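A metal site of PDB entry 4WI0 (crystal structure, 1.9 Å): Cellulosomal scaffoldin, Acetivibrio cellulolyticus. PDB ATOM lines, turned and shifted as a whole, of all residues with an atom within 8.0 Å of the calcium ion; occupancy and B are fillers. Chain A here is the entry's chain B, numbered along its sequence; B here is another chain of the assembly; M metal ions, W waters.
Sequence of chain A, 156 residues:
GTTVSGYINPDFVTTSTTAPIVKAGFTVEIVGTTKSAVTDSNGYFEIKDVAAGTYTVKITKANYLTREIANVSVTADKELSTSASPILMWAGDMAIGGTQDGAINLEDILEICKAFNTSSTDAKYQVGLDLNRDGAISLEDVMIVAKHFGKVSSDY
The side-chain carboxylate (OD2) of Asp 141 lies close to the backbone NH (N) of Ser 138 (2.8 Å).
N of Gly 135 of chain A lies within hydrogen-bond range of OD2 of Asp 130, 2.7 Å away.
OD2 of Asp 130 is in hydrogen-bond range of OH of Tyr 125 (2.6 Å).
The guanidinium group (NH1) of Arg 133 lies within hydrogen-bond range of the backbone carbonyl oxygen (O) of Asp 130.
The side-chain carboxylate (OD1) of Asp 141 lies close to the backbone NH (N) of Leu 131 (3.1 Å).
The side-chain carboxylate of Glu 140 lies within hydrogen-bond range of the side-chain amide nitrogen of Asn 132.
Water W1 lies within hydrogen-bond range of the side-chain hydroxyl (OG) of Ser 138 (2.6 Å) and the side-chain carboxylate (OD2) of Asp 134 (2.7 Å).
The calcium ion is bound by the side-chain amide oxygen (OD1) of Asn 132 (2.3 Å), the backbone carbonyl oxygen (O) of Ala 136 (2.4 Å), the side-chain carboxylate (OD1) of Asp 130 (2.4 Å), the side-chain carboxylate (OD1) of Asp 134 (2.4 Å), water W1 (2.4 Å), the side-chain carboxylate (OD1) of Asp 141 (2.4 Å) and the side-chain carboxylate (OD2) of Asp 141 (2.6 Å).
The calcium ion has seven donor atoms within binding distance.
Within 4 Å of the calcium ion: Asp 130, Asn 132, Asp 134, Ala 136 and Asp 141.
The nearest printed residue that does not touch the calcium ion is Ile 137 of chain A (4.4 Å).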
ATOM      1  N   THR A  18      17.192 -11.167 -25.279  1.00  0.00           N
ATOM      2  CA  THR A  18      18.054 -10.184 -24.605  1.00  0.00           C
ATOM      3  C   THR A  18      17.549  -8.738 -24.692  1.00  0.00           C
ATOM      4  O   THR A  18      17.805  -7.953 -23.797  1.00  0.00           O
ATOM      5  CB  THR A  18      19.506 -10.197 -25.151  1.00  0.00           C
ATOM      6  OG1 THR A  18      19.513  -9.755 -26.509  1.00  0.00           O
ATOM      7  CG2 THR A  18      20.104 -11.598 -25.066  1.00  0.00           C
ATOM      8  N   ILE A 112      36.190  -6.362 -17.667  1.00  0.00           N
ATOM      9  CA  ILE A 112      35.427  -7.475 -18.239  1.00  0.00           C
ATOM     10  C   ILE A 112      36.272  -8.760 -18.270  1.00  0.00           C
ATOM     11  O   ILE A 112      35.781  -9.851 -17.965  1.00  0.00           O
ATOM     12  CB  ILE A 112      34.913  -7.128 -19.653  1.00  0.00           C
ATOM     13  CG1 ILE A 112      33.878  -6.000 -19.578  1.00  0.00           C
ATOM     14  CG2 ILE A 112      34.290  -8.351 -20.324  1.00  0.00           C
ATOM     15  CD1 ILE A 112      33.678  -5.254 -20.877  1.00  0.00           C
ATOM     16  N   THR A 118      33.310 -17.098 -19.265  1.00  0.00           N
ATOM     17  CA  THR A 118      32.450 -17.699 -18.253  1.00  0.00           C
ATOM     18  C   THR A 118      31.004 -17.602 -18.701  1.00  0.00           C
ATOM     19  O   THR A 118      30.667 -16.779 -19.539  1.00  0.00           O
ATOM     20  CB  THR A 118      32.581 -17.000 -16.881  1.00  0.00           C
ATOM     21  OG1 THR A 118      32.314 -15.605 -17.028  1.00  0.00           O
ATOM     22  CG2 THR A 118      33.990 -17.182 -16.306  1.00  0.00           C
ATOM     23  N   TYR A 125      31.411 -15.599 -12.899  1.00  0.00           N
ATOM     24  CA  TYR A 125      30.590 -14.743 -13.747  1.00  0.00           C
ATOM     25  C   TYR A 125      29.897 -13.627 -12.959  1.00  0.00           C
ATOM     26  O   TYR A 125      29.334 -13.853 -11.896  1.00  0.00           O
ATOM     27  CB  TYR A 125      29.558 -15.605 -14.462  1.00  0.00           C
ATOM     28  CG  TYR A 125      28.490 -14.871 -15.237  1.00  0.00           C
ATOM     29  CD1 TYR A 125      27.364 -14.349 -14.602  1.00  0.00           C
ATOM     30  CD2 TYR A 125      28.563 -14.749 -16.624  1.00  0.00           C
ATOM     31  CE1 TYR A 125      26.369 -13.706 -15.306  1.00  0.00           C
ATOM     32  CE2 TYR A 125      27.573 -14.094 -17.346  1.00  0.00           C
ATOM     33  CZ  TYR A 125      26.479 -13.589 -16.675  1.00  0.00           C
ATOM     34  OH  TYR A 125      25.489 -12.940 -17.368  1.00  0.00           O
ATOM     35  N   VAL A 127      27.024 -10.623 -13.762  1.00  0.00           N
ATOM     36  CA  VAL A 127      26.063 -10.185 -14.776  1.00  0.00           C
ATOM     37  C   VAL A 127      26.396  -8.808 -15.373  1.00  0.00           C
ATOM     38  O   VAL A 127      26.169  -8.567 -16.553  1.00  0.00           O
ATOM     39  CB  VAL A 127      24.607 -10.232 -14.232  1.00  0.00           C
ATOM     40  CG1 VAL A 127      24.370  -9.149 -13.188  1.00  0.00           C
ATOM     41  CG2 VAL A 127      23.604 -10.104 -15.372  1.00  0.00           C
ATOM     42  N   LEU A 129      29.276  -7.593 -16.151  1.00  0.00           N
ATOM     43  CA  LEU A 129      30.336  -7.694 -17.155  1.00  0.00           C
ATOM     44  C   LEU A 129      29.813  -8.317 -18.458  1.00  0.00           C
ATOM     45  O   LEU A 129      30.418  -8.172 -19.518  1.00  0.00           O
ATOM     46  CB  LEU A 129      31.506  -8.524 -16.608  1.00  0.00           C
ATOM     47  CG  LEU A 129      32.084  -8.065 -15.249  1.00  0.00           C
ATOM     48  CD1 LEU A 129      33.257  -8.953 -14.868  1.00  0.00           C
ATOM     49  CD2 LEU A 129      32.509  -6.616 -15.261  1.00  0.00           C
ATOM     50  N   ASP A 130      28.672  -9.017 -18.348  1.00  0.00           N
ATOM     51  CA  ASP A 130      27.954  -9.552 -19.493  1.00  0.00           C
ATOM     52  C   ASP A 130      27.131  -8.422 -20.119  1.00  0.00           C
ATOM     53  O   ASP A 130      25.936  -8.305 -19.865  1.00  0.00           O
ATOM     54  CB  ASP A 130      27.060 -10.726 -19.041  1.00  0.00           C
ATOM     55  CG  ASP A 130      26.256 -11.349 -20.182  1.00  0.00           C
ATOM     56  OD1 ASP A 130      26.431 -10.929 -21.346  1.00  0.00           O
ATOM     57  OD2 ASP A 130      25.466 -12.277 -19.906  1.00  0.00           O
ATOM     58  N   LEU A 131      27.797  -7.602 -20.937  1.00  0.00           N
ATOM     59  CA  LEU A 131      27.209  -6.382 -21.499  1.00  0.00           C
ATOM     60  C   LEU A 131      25.967  -6.646 -22.358  1.00  0.00           C
ATOM     61  O   LEU A 131      24.985  -5.937 -22.209  1.00  0.00           O
ATOM     62  CB  LEU A 131      28.247  -5.599 -22.305  1.00  0.00           C
ATOM     63  CG  LEU A 131      29.444  -5.046 -21.527  1.00  0.00           C
ATOM     64  CD1 LEU A 131      30.336  -4.202 -22.417  1.00  0.00           C
ATOM     65  CD2 LEU A 131      28.969  -4.230 -20.338  1.00  0.00           C
ATOM     66  N   ASN A 132      26.016  -7.635 -23.233  1.00  0.00           N
ATOM     67  CA  ASN A 132      24.854  -7.950 -24.074  1.00  0.00           C
ATOM     68  C   ASN A 132      23.829  -8.897 -23.447  1.00  0.00           C
ATOM     69  O   ASN A 132      22.864  -9.294 -24.096  1.00  0.00           O
ATOM     70  CB  ASN A 132      25.286  -8.456 -25.472  1.00  0.00           C
ATOM     71  CG  ASN A 132      26.011  -9.800 -25.451  1.00  0.00           C
ATOM     72  OD1 ASN A 132      26.205 -10.409 -24.389  1.00  0.00           O
ATOM     73  ND2 ASN A 132      26.452 -10.230 -26.619  1.00  0.00           N
ATOM     74  N   ARG A 133      24.060  -9.258 -22.181  1.00  0.00           N
ATOM     75  CA  ARG A 133      23.179 -10.132 -21.379  1.00  0.00           C
ATOM     76  C   ARG A 133      22.778 -11.440 -22.064  1.00  0.00           C
ATOM     77  O   ARG A 133      21.641 -11.901 -21.903  1.00  0.00           O
ATOM     78  CB  ARG A 133      21.948  -9.353 -20.891  1.00  0.00           C
ATOM     79  CG  ARG A 133      22.271  -8.230 -19.916  1.00  0.00           C
ATOM     80  CD  ARG A 133      22.876  -8.737 -18.610  1.00  0.00           C
ATOM     81  NE  ARG A 133      22.860  -7.688 -17.579  1.00  0.00           N
ATOM     82  CZ  ARG A 133      23.696  -6.661 -17.498  1.00  0.00           C
ATOM     83  NH1 ARG A 133      24.683  -6.491 -18.391  1.00  0.00           N
ATOM     84  NH2 ARG A 133      23.564  -5.783 -16.511  1.00  0.00           N
ATOM     85  N   ASP A 134      23.703 -12.046 -22.802  1.00  0.00           N
ATOM     86  CA  ASP A 134      23.432 -13.364 -23.411  1.00  0.00           C
ATOM     87  C   ASP A 134      23.795 -14.537 -22.494  1.00  0.00           C
ATOM     88  O   ASP A 134      23.747 -15.690 -22.921  1.00  0.00           O
ATOM     89  CB  ASP A 134      24.093 -13.515 -24.791  1.00  0.00           C
ATOM     90  CG  ASP A 134      25.638 -13.458 -24.743  1.00  0.00           C
ATOM     91  OD1 ASP A 134      26.251 -13.338 -23.651  1.00  0.00           O
ATOM     92  OD2 ASP A 134      26.237 -13.542 -25.831  1.00  0.00           O
ATOM     93  N   GLY A 135      24.156 -14.236 -21.244  1.00  0.00           N
ATOM     94  CA  GLY A 135      24.447 -15.270 -20.245  1.00  0.00           C
ATOM     95  C   GLY A 135      25.865 -15.803 -20.307  1.00  0.00           C
ATOM     96  O   GLY A 135      26.161 -16.857 -19.752  1.00  0.00           O
ATOM     97  N   ALA A 136      26.745 -15.066 -20.984  1.00  0.00           N
ATOM     98  CA  ALA A 136      28.151 -15.426 -21.112  1.00  0.00           C
ATOM     99  C   ALA A 136      28.999 -14.158 -21.154  1.00  0.00           C
ATOM    100  O   ALA A 136      28.522 -13.098 -21.570  1.00  0.00           O
ATOM    101  CB  ALA A 136      28.370 -16.256 -22.358  1.00  0.00           C
ATOM    102  N   ILE A 137      30.241 -14.276 -20.725  1.00  0.00           N
ATOM    103  CA  ILE A 137      31.221 -13.201 -20.863  1.00  0.00           C
ATOM    104  C   ILE A 137      32.245 -13.747 -21.837  1.00  0.00           C
ATOM    105  O   ILE A 137      32.987 -14.671 -21.513  1.00  0.00           O
ATOM    106  CB  ILE A 137      31.856 -12.780 -19.524  1.00  0.00           C
ATOM    107  CG1 ILE A 137      30.764 -12.255 -18.573  1.00  0.00           C
ATOM    108  CG2 ILE A 137      32.892 -11.690 -19.753  1.00  0.00           C
ATOM    109  CD1 ILE A 137      31.174 -12.181 -17.118  1.00  0.00           C
ATOM    110  N   SER A 138      32.240 -13.185 -23.047  1.00  0.00           N
ATOM    111  CA  SER A 138      33.006 -13.727 -24.166  1.00  0.00           C
ATOM    112  C   SER A 138      33.567 -12.565 -24.979  1.00  0.00           C
ATOM    113  O   SER A 138      33.474 -11.419 -24.560  1.00  0.00           O
ATOM    114  CB  SER A 138      32.101 -14.616 -25.034  1.00  0.00           C
ATOM    115  OG  SER A 138      30.994 -13.913 -25.558  1.00  0.00           O
ATOM    116  N   LEU A 139      34.159 -12.869 -26.145  1.00  0.00           N
ATOM    117  CA  LEU A 139      34.755 -11.826 -26.995  1.00  0.00           C
ATOM    118  C   LEU A 139      33.719 -10.806 -27.474  1.00  0.00           C
ATOM    119  O   LEU A 139      34.055  -9.643 -27.688  1.00  0.00           O
ATOM    120  CB  LEU A 139      35.477 -12.446 -28.190  1.00  0.00           C
ATOM    121  CG  LEU A 139      36.279 -11.485 -29.084  1.00  0.00           C
ATOM    122  CD1 LEU A 139      37.221 -10.602 -28.260  1.00  0.00           C
ATOM    123  CD2 LEU A 139      37.062 -12.268 -30.122  1.00  0.00           C
ATOM    124  N   GLU A 140      32.463 -11.228 -27.650  1.00  0.00           N
ATOM    125  CA  GLU A 140      31.389 -10.289 -28.023  1.00  0.00           C
ATOM    126  C   GLU A 140      31.299  -9.092 -27.092  1.00  0.00           C
ATOM    127  O   GLU A 140      31.175  -7.959 -27.543  1.00  0.00           O
ATOM    128  CB  GLU A 140      30.041 -10.988 -28.040  1.00  0.00           C
ATOM    129  CG  GLU A 140      29.860 -11.872 -29.234  1.00  0.00           C
ATOM    130  CD  GLU A 140      28.572 -12.637 -29.205  1.00  0.00           C
ATOM    131  OE1 GLU A 140      27.509 -11.957 -29.183  1.00  0.00           O
ATOM    132  OE2 GLU A 140      28.638 -13.893 -29.207  1.00  0.00           O
ATOM    133  N   ASP A 141      31.356  -9.357 -25.789  1.00  0.00           N
ATOM    134  CA  ASP A 141      31.281  -8.300 -24.776  1.00  0.00           C
ATOM    135  C   ASP A 141      32.461  -7.350 -24.895  1.00  0.00           C
ATOM    136  O   ASP A 141      32.301  -6.140 -24.818  1.00  0.00           O
ATOM    137  CB  ASP A 141      31.259  -8.915 -23.372  1.00  0.00           C
ATOM    138  CG  ASP A 141      30.087  -9.870 -23.192  1.00  0.00           C
ATOM    139  OD1 ASP A 141      28.943  -9.396 -23.160  1.00  0.00           O
ATOM    140  OD2 ASP A 141      30.334 -11.095 -23.132  1.00  0.00           O
ATOM    141  N   VAL A 142      33.648  -7.909 -25.110  1.00  0.00           N
ATOM    142  CA  VAL A 142      34.867  -7.116 -25.284  1.00  0.00           C
ATOM    143  C   VAL A 142      34.794  -6.265 -26.564  1.00  0.00           C
ATOM    144  O   VAL A 142      35.183  -5.084 -26.550  1.00  0.00           O
ATOM    145  CB  VAL A 142      36.125  -8.030 -25.300  1.00  0.00           C
ATOM    146  CG1 VAL A 142      37.366  -7.270 -25.778  1.00  0.00           C
ATOM    147  CG2 VAL A 142      36.352  -8.636 -23.921  1.00  0.00           C
ATOM    148  N   ILE A 144      32.128  -5.145 -28.049  1.00  0.00           N
ATOM    149  CA  ILE A 144      31.158  -4.068 -27.833  1.00  0.00           C
ATOM    150  C   ILE A 144      31.872  -2.825 -27.284  1.00  0.00           C
ATOM    151  O   ILE A 144      31.615  -1.707 -27.734  1.00  0.00           O
ATOM    152  CB  ILE A 144      30.026  -4.497 -26.868  1.00  0.00           C
ATOM    153  CG1 ILE A 144      29.089  -5.456 -27.576  1.00  0.00           C
ATOM    154  CG2 ILE A 144      29.235  -3.294 -26.355  1.00  0.00           C
ATOM    155  CD1 ILE A 144      28.138  -6.166 -26.635  1.00  0.00           C
ATOM    156  N   THR B 135      30.011 -21.127 -22.957  1.00  0.00           N
ATOM    157  CA  THR B 135      30.608 -19.816 -22.779  1.00  0.00           C
ATOM    158  C   THR B 135      30.600 -18.975 -24.063  1.00  0.00           C
ATOM    159  O   THR B 135      30.968 -17.794 -24.028  1.00  0.00           O
ATOM    160  CB  THR B 135      32.077 -19.928 -22.273  1.00  0.00           C
ATOM    161  OG1 THR B 135      32.899 -20.505 -23.288  1.00  0.00           O
ATOM    162  CG2 THR B 135      32.157 -20.772 -20.992  1.00  0.00           C
ATOM    163  N   PRO B 137      27.718 -18.389 -26.595  1.00  0.00           N
ATOM    164  CA  PRO B 137      26.310 -18.620 -26.920  1.00  0.00           C
ATOM    165  C   PRO B 137      25.982 -18.760 -28.413  1.00  0.00           C
ATOM    166  O   PRO B 137      25.215 -19.633 -28.780  1.00  0.00           O
ATOM    167  CB  PRO B 137      25.619 -17.378 -26.340  1.00  0.00           C
ATOM    168  CG  PRO B 137      26.457 -17.012 -25.172  1.00  0.00           C
ATOM    169  CD  PRO B 137      27.868 -17.354 -25.542  1.00  0.00           C
HETATM  170 CA    CA M   1      27.817 -11.561 -23.208  1.00  0.00          CA
HETATM  171  O   HOH W   1      28.755 -12.745 -25.122  1.00  0.00           O
